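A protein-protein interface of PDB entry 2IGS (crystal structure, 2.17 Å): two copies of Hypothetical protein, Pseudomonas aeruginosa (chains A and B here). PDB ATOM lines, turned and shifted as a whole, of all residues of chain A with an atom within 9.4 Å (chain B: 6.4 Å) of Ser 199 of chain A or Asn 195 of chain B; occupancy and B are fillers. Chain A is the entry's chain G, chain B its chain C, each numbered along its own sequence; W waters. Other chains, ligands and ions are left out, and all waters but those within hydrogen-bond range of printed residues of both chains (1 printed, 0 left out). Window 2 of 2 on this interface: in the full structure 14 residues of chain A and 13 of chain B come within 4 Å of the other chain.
The backbone carbonyl oxygen (O) of Val 132 of chain A sits at hydrogen-bond distance from the side-chain hydroxyl (OG) of Ser 191 of chain B (2.8 Å). The side-chain carboxylate (OD1) of Asp 192 of chain B lies within salt-bridge range of the side-chain amino group (NZ) of Lys 198 of chain A, 2.9 Å away. ND2 of Asn 195 of chain B lies within hydrogen-bond range of OD1 of Asn 195 of chain A, at 3.4 Å. The side-chain hydroxyl (OG) of Ser 199 of chain B sits at hydrogen-bond distance from the side-chain amide oxygen (OD1) of Asn 195 of chain A. NZ of Lys 198 of chain B lies within salt-bridge range of OD1 of Asp 192 of chain A (2.5 Å). The side-chain amide nitrogen (ND2) of Asn 195 of chain B sits at hydrogen-bond distance from the side-chain hydroxyl (OG) of Ser 199 of chain A (3.3 Å). The side-chain amino group (NZ) of Lys 198 of chain A sits close to the side-chain hydroxyl (OG) of Ser 191 of chain B (3.3 Å).
The backbone carbonyl oxygen (O) of Asp 192 of chain B is in hydrogen-bond range of the side-chain hydroxyl (OG1) of Thr 196 of chain B (3.0 Å). O of Asn 195 of chain B sits at hydrogen-bond distance from OG of Ser 199 of chain B. The backbone carbonyl oxygen (O) of Asn 195 of chain A is in hydrogen-bond range of the side-chain hydroxyl (OG) of Ser 199 of chain A (3.0 Å). The backbone carbonyl oxygen (O) of Asp 192 of chain A sits at hydrogen-bond distance from the side-chain hydroxyl (OG1) of Thr 196 of chain A, 2.9 Å away.
CE2 of Phe 190 of chain B touches CE1 of Phe 134 of chain A, 3.7 Å away. CZ of Phe 194 of chain B touches OG of Ser 191 of chain A, 3.1 Å away. Lys 198 of chain B touches Ser 191 of chain A. Phe 194 of chain A touches Ser 191 of chain B (CE1 to OG, 3.3 Å). Asn 195 of chain A touches Lys 198 of chain B (OD1 to CD, 3.7 Å). Lys 198 of chain A touches Asn 195 of chain B (CD to CB, 3.7 Å).
Of chain B, only Asn 195 comes within 4 Å of Ser 199 of chain A. Of the printed residues of chain A, Asn 195 of chain B touches Asn 195 (3.4 Å), Lys 198 (3.7 Å) and Ser 199 (3.3 Å). No residue of chain A comes within 4 Å of Thr 196 of chain B. Of the printed residues of chain B, Val 132 of chain A touches Ser 191 (2.8 Å). Of the printed residues of chain B, Asp 192 of chain A touches Lys 198. Printed residues of chain B within 4 Å of Asn 195 of chain A: Asn 195 (3.4 Å), Lys 198 (3.7 Å) and Ser 199 (3.3 Å). Of the printed residues of chain B, Lys 198 of chain A touches Ser 191 (3.2 Å), Asp 192 (2.9 Å) and Asn 195 (3.7 Å).
Hydrophobic or aromatic side chains of chain B within 4 Å of the printed part of chain A: Phe 190 and Phe 194. Of the 20 printed residues of chain A, 8 touch a printed residue of chain B. Printed residues of chain A that touch a printed residue of chain B: Val 132, Phe 134, Ser 191, Asp 192, Phe 194, Asn 195, Lys 198 and Ser 199. Hydrophobic or aromatic side chains of chain A within 4 Å of the printed part of chain B: Phe 134 and Phe 194. Among the printed residues, 13 pairs touch across the chains. Among the printed residues, Asp or Glu carboxylates within 4 Å of a Lys or Arg side-chain nitrogen of the other chain: Asp 192 of chain A with Lys 198 of chain B and Lys 198 of chain A with Asp 192 of chain B.
Ser 191 of chain A touches Phe 194 of chain B, and with the chains exchanged Phe 194 of chain A touches Ser 191 of chain B. Ser 191 of chain A touches Lys 198 of chain B, and with the chains exchanged Lys 198 of chain A touches Ser 191 of chain B. Asp 192 of chain A touches Lys 198 of chain B, and with the chains exchanged Lys 198 of chain A touches Asp 192 of chain B. Asn 195 of chain A touches Ser 199 of chain B, and with the chains exchanged Ser 199 of chain A touches Asn 195 of chain B. Positions printed for both chains: 191, 192, 193, 194, 195, 196, 197, 198, 199 and 200. Of the 13 pairs that touch across the chains among the printed residues, 11 have their exchanged pair printed and touching as well.
Water W1 lies within hydrogen-bond range of the backbone NH (N) of Val 132 of chain A (2.9 Å), the side-chain amino group (NZ) of Lys 198 of chain A (3.1 Å), the side-chain carboxylate (OD1) of Asp 131 of chain A (3.2 Å) and the side-chain hydroxyl (OG) of Ser 191 of chain B (3.2 Å).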
ATOM      1  N   GLN A  71      13.445  -5.343 -35.109  1.00  0.00           N
ATOM      2  CA  GLN A  71      12.538  -4.252 -35.486  1.00  0.00           C
ATOM      3  C   GLN A  71      13.185  -3.211 -36.396  1.00  0.00           C
ATOM      4  O   GLN A  71      12.555  -2.754 -37.358  1.00  0.00           O
ATOM      5  CB  GLN A  71      12.016  -3.528 -34.266  1.00  0.00           C
ATOM      6  CG  GLN A  71      10.807  -4.135 -33.625  1.00  0.00           C
ATOM      7  CD  GLN A  71      10.434  -3.399 -32.332  1.00  0.00           C
ATOM      8  OE1 GLN A  71      10.898  -2.251 -32.065  1.00  0.00           O
ATOM      9  NE2 GLN A  71       9.590  -4.048 -31.522  1.00  0.00           N
ATOM     10  N   THR A 130      13.718   1.924 -25.533  1.00  0.00           N
ATOM     11  CA  THR A 130      12.359   2.115 -26.010  1.00  0.00           C
ATOM     12  C   THR A 130      11.299   2.025 -24.899  1.00  0.00           C
ATOM     13  O   THR A 130      10.108   2.148 -25.179  1.00  0.00           O
ATOM     14  CB  THR A 130      12.047   1.032 -27.045  1.00  0.00           C
ATOM     15  OG1 THR A 130      12.535  -0.212 -26.546  1.00  0.00           O
ATOM     16  CG2 THR A 130      12.753   1.331 -28.361  1.00  0.00           C
ATOM     17  N   ASP A 131      11.730   1.789 -23.655  1.00  0.00           N
ATOM     18  CA  ASP A 131      10.813   1.670 -22.537  1.00  0.00           C
ATOM     19  C   ASP A 131       9.986   2.935 -22.315  1.00  0.00           C
ATOM     20  O   ASP A 131      10.447   4.059 -22.560  1.00  0.00           O
ATOM     21  CB  ASP A 131      11.529   1.291 -21.254  1.00  0.00           C
ATOM     22  CG  ASP A 131      11.919  -0.189 -21.201  1.00  0.00           C
ATOM     23  OD1 ASP A 131      11.333  -0.998 -21.946  1.00  0.00           O
ATOM     24  OD2 ASP A 131      12.833  -0.540 -20.405  1.00  0.00           O
ATOM     25  N   VAL A 132       8.733   2.707 -21.919  1.00  0.00           N
ATOM     26  CA  VAL A 132       7.821   3.738 -21.507  1.00  0.00           C
ATOM     27  C   VAL A 132       7.295   3.239 -20.171  1.00  0.00           C
ATOM     28  O   VAL A 132       6.689   2.173 -20.087  1.00  0.00           O
ATOM     29  CB  VAL A 132       6.649   3.940 -22.518  1.00  0.00           C
ATOM     30  CG1 VAL A 132       5.737   5.036 -22.024  1.00  0.00           C
ATOM     31  CG2 VAL A 132       7.174   4.340 -23.891  1.00  0.00           C
ATOM     32  N   PHE A 134       6.444   4.963 -15.860  1.00  0.00           N
ATOM     33  CA  PHE A 134       5.853   6.049 -15.079  1.00  0.00           C
ATOM     34  C   PHE A 134       6.918   6.916 -14.413  1.00  0.00           C
ATOM     35  O   PHE A 134       7.904   6.406 -13.874  1.00  0.00           O
ATOM     36  CB  PHE A 134       4.918   5.470 -14.013  1.00  0.00           C
ATOM     37  CG  PHE A 134       3.772   4.714 -14.578  1.00  0.00           C
ATOM     38  CD1 PHE A 134       3.763   3.325 -14.555  1.00  0.00           C
ATOM     39  CD2 PHE A 134       2.699   5.392 -15.173  1.00  0.00           C
ATOM     40  CE1 PHE A 134       2.695   2.599 -15.107  1.00  0.00           C
ATOM     41  CE2 PHE A 134       1.601   4.681 -15.724  1.00  0.00           C
ATOM     42  CZ  PHE A 134       1.609   3.277 -15.696  1.00  0.00           C
ATOM     43  N   LEU A 176       5.033  12.528 -32.157  1.00  0.00           N
ATOM     44  CA  LEU A 176       4.748  11.350 -31.310  1.00  0.00           C
ATOM     45  C   LEU A 176       4.677  11.687 -29.808  1.00  0.00           C
ATOM     46  O   LEU A 176       3.755  11.279 -29.094  1.00  0.00           O
ATOM     47  CB  LEU A 176       5.834  10.267 -31.510  1.00  0.00           C
ATOM     48  CG  LEU A 176       5.663   8.908 -30.818  1.00  0.00           C
ATOM     49  CD1 LEU A 176       4.407   8.202 -31.318  1.00  0.00           C
ATOM     50  CD2 LEU A 176       6.895   8.047 -31.080  1.00  0.00           C
ATOM     51  N   SER A 191      -3.930   7.022 -21.369  1.00  0.00           N
ATOM     52  CA  SER A 191      -3.795   5.648 -21.875  1.00  0.00           C
ATOM     53  C   SER A 191      -3.453   5.588 -23.336  1.00  0.00           C
ATOM     54  O   SER A 191      -2.593   4.790 -23.727  1.00  0.00           O
ATOM     55  CB  SER A 191      -5.088   4.862 -21.690  1.00  0.00           C
ATOM     56  OG  SER A 191      -4.984   4.144 -20.499  1.00  0.00           O
ATOM     57  N   ASP A 192      -4.186   6.386 -24.123  1.00  0.00           N
ATOM     58  CA  ASP A 192      -3.972   6.521 -25.557  1.00  0.00           C
ATOM     59  C   ASP A 192      -2.571   6.994 -25.865  1.00  0.00           C
ATOM     60  O   ASP A 192      -1.930   6.427 -26.736  1.00  0.00           O
ATOM     61  CB  ASP A 192      -4.976   7.506 -26.184  1.00  0.00           C
ATOM     62  CG  ASP A 192      -6.354   6.891 -26.409  1.00  0.00           C
ATOM     63  OD1 ASP A 192      -6.532   5.705 -26.079  1.00  0.00           O
ATOM     64  OD2 ASP A 192      -7.270   7.595 -26.906  1.00  0.00           O
ATOM     65  N   VAL A 193      -2.117   8.042 -25.171  1.00  0.00           N
ATOM     66  CA  VAL A 193      -0.831   8.684 -25.469  1.00  0.00           C
ATOM     67  C   VAL A 193       0.291   7.750 -25.055  1.00  0.00           C
ATOM     68  O   VAL A 193       1.218   7.533 -25.827  1.00  0.00           O
ATOM     69  CB  VAL A 193      -0.679  10.063 -24.741  1.00  0.00           C
ATOM     70  CG1 VAL A 193       0.746  10.600 -24.853  1.00  0.00           C
ATOM     71  CG2 VAL A 193      -1.725  11.096 -25.252  1.00  0.00           C
ATOM     72  N   PHE A 194       0.187   7.192 -23.842  1.00  0.00           N
ATOM     73  CA  PHE A 194       1.096   6.150 -23.374  1.00  0.00           C
ATOM     74  C   PHE A 194       1.295   5.068 -24.425  1.00  0.00           C
ATOM     75  O   PHE A 194       2.416   4.757 -24.769  1.00  0.00           O
ATOM     76  CB  PHE A 194       0.564   5.497 -22.089  1.00  0.00           C
ATOM     77  CG  PHE A 194       1.541   4.546 -21.409  1.00  0.00           C
ATOM     78  CD1 PHE A 194       1.920   3.343 -22.001  1.00  0.00           C
ATOM     79  CD2 PHE A 194       2.040   4.838 -20.126  1.00  0.00           C
ATOM     80  CE1 PHE A 194       2.804   2.460 -21.363  1.00  0.00           C
ATOM     81  CE2 PHE A 194       2.933   3.946 -19.471  1.00  0.00           C
ATOM     82  CZ  PHE A 194       3.299   2.748 -20.105  1.00  0.00           C
ATOM     83  N   ASN A 195       0.174   4.473 -24.861  1.00  0.00           N
ATOM     84  CA  ASN A 195       0.094   3.361 -25.837  1.00  0.00           C
ATOM     85  C   ASN A 195       0.711   3.748 -27.176  1.00  0.00           C
ATOM     86  O   ASN A 195       1.522   3.007 -27.728  1.00  0.00           O
ATOM     87  CB  ASN A 195      -1.378   2.908 -26.014  1.00  0.00           C
ATOM     88  CG  ASN A 195      -1.573   1.796 -27.087  1.00  0.00           C
ATOM     89  OD1 ASN A 195      -1.782   0.623 -26.764  1.00  0.00           O
ATOM     90  ND2 ASN A 195      -1.541   2.187 -28.362  1.00  0.00           N
ATOM     91  N   THR A 196       0.318   4.918 -27.676  1.00  0.00           N
ATOM     92  CA  THR A 196       0.856   5.491 -28.919  1.00  0.00           C
ATOM     93  C   THR A 196       2.395   5.697 -28.886  1.00  0.00           C
ATOM     94  O   THR A 196       3.089   5.397 -29.876  1.00  0.00           O
ATOM     95  CB  THR A 196       0.124   6.811 -29.267  1.00  0.00           C
ATOM     96  OG1 THR A 196      -1.240   6.494 -29.542  1.00  0.00           O
ATOM     97  CG2 THR A 196       0.702   7.451 -30.495  1.00  0.00           C
ATOM     98  N   ILE A 197       2.922   6.205 -27.776  1.00  0.00           N
ATOM     99  CA  ILE A 197       4.359   6.414 -27.670  1.00  0.00           C
ATOM    100  C   ILE A 197       5.093   5.081 -27.523  1.00  0.00           C
ATOM    101  O   ILE A 197       6.094   4.860 -28.188  1.00  0.00           O
ATOM    102  CB  ILE A 197       4.766   7.401 -26.529  1.00  0.00           C
ATOM    103  CG1 ILE A 197       4.169   8.813 -26.759  1.00  0.00           C
ATOM    104  CG2 ILE A 197       6.276   7.456 -26.401  1.00  0.00           C
ATOM    105  CD1 ILE A 197       4.301   9.764 -25.537  1.00  0.00           C
ATOM    106  N   LYS A 198       4.585   4.191 -26.672  1.00  0.00           N
ATOM    107  CA  LYS A 198       5.139   2.840 -26.565  1.00  0.00           C
ATOM    108  C   LYS A 198       5.208   2.095 -27.902  1.00  0.00           C
ATOM    109  O   LYS A 198       6.208   1.434 -28.176  1.00  0.00           O
ATOM    110  CB  LYS A 198       4.366   1.990 -25.564  1.00  0.00           C
ATOM    111  CG  LYS A 198       5.140   0.714 -25.245  1.00  0.00           C
ATOM    112  CD  LYS A 198       4.482  -0.144 -24.242  1.00  0.00           C
ATOM    113  CE  LYS A 198       5.205  -1.474 -24.191  1.00  0.00           C
ATOM    114  NZ  LYS A 198       6.581  -1.405 -23.600  1.00  0.00           N
ATOM    115  N   SER A 199       4.157   2.192 -28.717  1.00  0.00           N
ATOM    116  CA  SER A 199       4.097   1.480 -30.008  1.00  0.00           C
ATOM    117  C   SER A 199       4.885   2.172 -31.107  1.00  0.00           C
ATOM    118  O   SER A 199       5.322   1.536 -32.054  1.00  0.00           O
ATOM    119  CB  SER A 199       2.642   1.331 -30.492  1.00  0.00           C
ATOM    120  OG  SER A 199       1.866   0.644 -29.525  1.00  0.00           O
ATOM    121  N   GLY A 200       5.032   3.485 -30.994  1.00  0.00           N
ATOM    122  CA  GLY A 200       5.700   4.297 -32.022  1.00  0.00           C
ATOM    123  C   GLY A 200       7.222   4.368 -31.956  1.00  0.00           C
ATOM    124  O   GLY A 200       7.872   4.684 -32.953  1.00  0.00           O
ATOM    125  N   LEU A 201       7.792   4.070 -30.796  1.00  0.00           N
ATOM    126  CA  LEU A 201       9.237   4.157 -30.631  1.00  0.00           C
ATOM    127  C   LEU A 201       9.960   2.959 -31.209  1.00  0.00           C
ATOM    128  O   LEU A 201       9.436   1.842 -31.222  1.00  0.00           O
ATOM    129  CB  LEU A 201       9.622   4.353 -29.159  1.00  0.00           C
ATOM    130  CG  LEU A 201       9.362   5.758 -28.588  1.00  0.00           C
ATOM    131  CD1 LEU A 201       9.729   5.793 -27.120  1.00  0.00           C
ATOM    132  CD2 LEU A 201      10.126   6.861 -29.375  1.00  0.00           C
ATOM    133  N   ARG A 202      11.158   3.228 -31.720  1.00  0.00           N
ATOM    134  CA  ARG A 202      12.081   2.210 -32.180  1.00  0.00           C
ATOM    135  C   ARG A 202      13.409   2.480 -31.486  1.00  0.00           C
ATOM    136  O   ARG A 202      13.636   3.565 -30.922  1.00  0.00           O
ATOM    137  CB  ARG A 202      12.252   2.292 -33.710  1.00  0.00           C
ATOM    138  CG  ARG A 202      11.104   1.639 -34.546  1.00  0.00           C
ATOM    139  CD  ARG A 202      10.923   2.297 -35.955  1.00  0.00           C
ATOM    140  NE  ARG A 202      12.217   2.786 -36.446  1.00  0.00           N
ATOM    141  CZ  ARG A 202      12.431   3.958 -37.042  1.00  0.00           C
ATOM    142  NH1 ARG A 202      11.420   4.796 -37.282  1.00  0.00           N
ATOM    143  NH2 ARG A 202      13.678   4.283 -37.415  1.00  0.00           N
ATOM    144  N   TYR A 203      14.303   1.501 -31.547  1.00  0.00           N
ATOM    145  CA  TYR A 203      15.625   1.624 -30.947  1.00  0.00           C
ATOM    146  C   TYR A 203      16.324   2.934 -31.339  1.00  0.00           C
ATOM    147  O   TYR A 203      16.770   3.698 -30.468  1.00  0.00           O
ATOM    148  CB  TYR A 203      16.454   0.402 -31.366  1.00  0.00           C
ATOM    149  CG  TYR A 203      17.863   0.332 -30.829  1.00  0.00           C
ATOM    150  CD1 TYR A 203      18.889   1.097 -31.399  1.00  0.00           C
ATOM    151  CD2 TYR A 203      18.190  -0.550 -29.787  1.00  0.00           C
ATOM    152  CE1 TYR A 203      20.197   1.006 -30.934  1.00  0.00           C
ATOM    153  CE2 TYR A 203      19.499  -0.657 -29.320  1.00  0.00           C
ATOM    154  CZ  TYR A 203      20.498   0.111 -29.901  1.00  0.00           C
ATOM    155  OH  TYR A 203      21.793   0.013 -29.435  1.00  0.00           O
ATOM    156  N   THR A 205      15.088   5.756 -32.951  1.00  0.00           N
ATOM    157  CA  THR A 205      14.325   6.973 -32.681  1.00  0.00           C
ATOM    158  C   THR A 205      14.165   7.274 -31.187  1.00  0.00           C
ATOM    159  O   THR A 205      13.979   8.431 -30.797  1.00  0.00           O
ATOM    160  CB  THR A 205      12.909   6.947 -33.350  1.00  0.00           C
ATOM    161  OG1 THR A 205      12.171   5.851 -32.827  1.00  0.00           O
ATOM    162  CG2 THR A 205      12.999   6.823 -34.894  1.00  0.00           C
ATOM    163  N   PHE B 190       4.878  -4.389 -16.661  1.00  0.00           N
ATOM    164  CA  PHE B 190       3.553  -3.734 -16.611  1.00  0.00           C
ATOM    165  C   PHE B 190       3.190  -2.977 -17.890  1.00  0.00           C
ATOM    166  O   PHE B 190       2.088  -3.121 -18.407  1.00  0.00           O
ATOM    167  CB  PHE B 190       3.353  -2.818 -15.396  1.00  0.00           C
ATOM    168  CG  PHE B 190       1.995  -2.146 -15.374  1.00  0.00           C
ATOM    169  CD1 PHE B 190       0.921  -2.758 -14.769  1.00  0.00           C
ATOM    170  CD2 PHE B 190       1.798  -0.925 -16.006  1.00  0.00           C
ATOM    171  CE1 PHE B 190      -0.325  -2.164 -14.761  1.00  0.00           C
ATOM    172  CE2 PHE B 190       0.561  -0.316 -16.008  1.00  0.00           C
ATOM    173  CZ  PHE B 190      -0.513  -0.937 -15.386  1.00  0.00           C
ATOM    174  N   SER B 191       4.119  -2.160 -18.377  1.00  0.00           N
ATOM    175  CA  SER B 191       3.959  -1.413 -19.636  1.00  0.00           C
ATOM    176  C   SER B 191       3.583  -2.318 -20.824  1.00  0.00           C
ATOM    177  O   SER B 191       2.624  -2.018 -21.568  1.00  0.00           O
ATOM    178  CB  SER B 191       5.236  -0.635 -19.929  1.00  0.00           C
ATOM    179  OG  SER B 191       5.104   0.161 -21.091  1.00  0.00           O
ATOM    180  N   ASP B 192       4.322  -3.420 -20.991  1.00  0.00           N
ATOM    181  CA  ASP B 192       4.026  -4.423 -22.025  1.00  0.00           C
ATOM    182  C   ASP B 192       2.617  -4.977 -21.918  1.00  0.00           C
ATOM    183  O   ASP B 192       1.890  -5.041 -22.913  1.00  0.00           O
ATOM    184  CB  ASP B 192       4.972  -5.614 -21.931  1.00  0.00           C
ATOM    185  CG  ASP B 192       6.344  -5.327 -22.476  1.00  0.00           C
ATOM    186  OD1 ASP B 192       6.649  -4.187 -22.902  1.00  0.00           O
ATOM    187  OD2 ASP B 192       7.148  -6.279 -22.468  1.00  0.00           O
ATOM    188  N   VAL B 193       2.258  -5.407 -20.709  1.00  0.00           N
ATOM    189  CA  VAL B 193       0.995  -6.075 -20.465  1.00  0.00           C
ATOM    190  C   VAL B 193      -0.160  -5.082 -20.643  1.00  0.00           C
ATOM    191  O   VAL B 193      -1.173  -5.409 -21.256  1.00  0.00           O
ATOM    192  CB  VAL B 193       0.964  -6.746 -19.051  1.00  0.00           C
ATOM    193  CG1 VAL B 193      -0.413  -7.258 -18.749  1.00  0.00           C
ATOM    194  CG2 VAL B 193       1.950  -7.898 -18.977  1.00  0.00           C
ATOM    195  N   PHE B 194       0.005  -3.873 -20.104  1.00  0.00           N
ATOM    196  CA  PHE B 194      -0.898  -2.753 -20.383  1.00  0.00           C
ATOM    197  C   PHE B 194      -1.148  -2.539 -21.889  1.00  0.00           C
ATOM    198  O   PHE B 194      -2.287  -2.429 -22.331  1.00  0.00           O
ATOM    199  CB  PHE B 194      -0.312  -1.465 -19.793  1.00  0.00           C
ATOM    200  CG  PHE B 194      -1.266  -0.318 -19.780  1.00  0.00           C
ATOM    201  CD1 PHE B 194      -1.602   0.345 -20.941  1.00  0.00           C
ATOM    202  CD2 PHE B 194      -1.836   0.109 -18.600  1.00  0.00           C
ATOM    203  CE1 PHE B 194      -2.493   1.414 -20.931  1.00  0.00           C
ATOM    204  CE2 PHE B 194      -2.735   1.190 -18.583  1.00  0.00           C
ATOM    205  CZ  PHE B 194      -3.045   1.838 -19.759  1.00  0.00           C
ATOM    206  N   ASN B 195      -0.059  -2.446 -22.647  1.00  0.00           N
ATOM    207  CA  ASN B 195      -0.066  -2.215 -24.086  1.00  0.00           C
ATOM    208  C   ASN B 195      -0.839  -3.315 -24.821  1.00  0.00           C
ATOM    209  O   ASN B 195      -1.713  -3.032 -25.650  1.00  0.00           O
ATOM    210  CB  ASN B 195       1.393  -2.125 -24.561  1.00  0.00           C
ATOM    211  CG  ASN B 195       1.539  -1.900 -26.061  1.00  0.00           C
ATOM    212  OD1 ASN B 195       1.854  -2.838 -26.810  1.00  0.00           O
ATOM    213  ND2 ASN B 195       1.343  -0.652 -26.507  1.00  0.00           N
ATOM    214  N   THR B 196      -0.542  -4.560 -24.467  1.00  0.00           N
ATOM    215  CA  THR B 196      -1.143  -5.722 -25.088  1.00  0.00           C
ATOM    216  C   THR B 196      -2.648  -5.737 -24.884  1.00  0.00           C
ATOM    217  O   THR B 196      -3.402  -5.885 -25.833  1.00  0.00           O
ATOM    218  CB  THR B 196      -0.524  -7.010 -24.532  1.00  0.00           C
ATOM    219  OG1 THR B 196       0.846  -7.059 -24.919  1.00  0.00           O
ATOM    220  CG2 THR B 196      -1.200  -8.236 -25.099  1.00  0.00           C
ATOM    221  N   ILE B 197      -3.081  -5.592 -23.637  1.00  0.00           N
ATOM    222  CA  ILE B 197      -4.490  -5.652 -23.316  1.00  0.00           C
ATOM    223  C   ILE B 197      -5.202  -4.496 -24.027  1.00  0.00           C
ATOM    224  O   ILE B 197      -6.251  -4.692 -24.644  1.00  0.00           O
ATOM    225  CB  ILE B 197      -4.717  -5.572 -21.788  1.00  0.00           C
ATOM    226  CG1 ILE B 197      -4.181  -6.836 -21.084  1.00  0.00           C
ATOM    227  CG2 ILE B 197      -6.162  -5.296 -21.492  1.00  0.00           C
ATOM    228  CD1 ILE B 197      -4.208  -6.756 -19.553  1.00  0.00           C
ATOM    229  N   LYS B 198      -4.627  -3.300 -23.953  1.00  0.00           N
ATOM    230  CA  LYS B 198      -5.245  -2.145 -24.600  1.00  0.00           C
ATOM    231  C   LYS B 198      -5.443  -2.358 -26.103  1.00  0.00           C
ATOM    232  O   LYS B 198      -6.504  -2.042 -26.637  1.00  0.00           O
ATOM    233  CB  LYS B 198      -4.433  -0.872 -24.383  1.00  0.00           C
ATOM    234  CG  LYS B 198      -5.256   0.349 -24.739  1.00  0.00           C
ATOM    235  CD  LYS B 198      -4.535   1.632 -24.460  1.00  0.00           C
ATOM    236  CE  LYS B 198      -5.534   2.763 -24.411  1.00  0.00           C
ATOM    237  NZ  LYS B 198      -5.544   3.384 -25.725  1.00  0.00           N
ATOM    238  N   SER B 199      -4.415  -2.898 -26.759  1.00  0.00           N
ATOM    239  CA  SER B 199      -4.424  -3.140 -28.193  1.00  0.00           C
ATOM    240  C   SER B 199      -5.295  -4.347 -28.580  1.00  0.00           C
ATOM    241  O   SER B 199      -5.714  -4.454 -29.732  1.00  0.00           O
ATOM    242  CB  SER B 199      -2.983  -3.357 -28.709  1.00  0.00           C
ATOM    243  OG  SER B 199      -2.182  -2.215 -28.481  1.00  0.00           O
ATOM    244  N   GLY B 200      -5.545  -5.241 -27.623  1.00  0.00           N
ATOM    245  CA  GLY B 200      -6.170  -6.521 -27.888  1.00  0.00           C
ATOM    246  C   GLY B 200      -7.683  -6.496 -27.789  1.00  0.00           C
ATOM    247  O   GLY B 200      -8.364  -7.272 -28.458  1.00  0.00           O
HETATM  248  O   HOH W   1       8.308  -0.139 -21.310  1.00  0.00           O
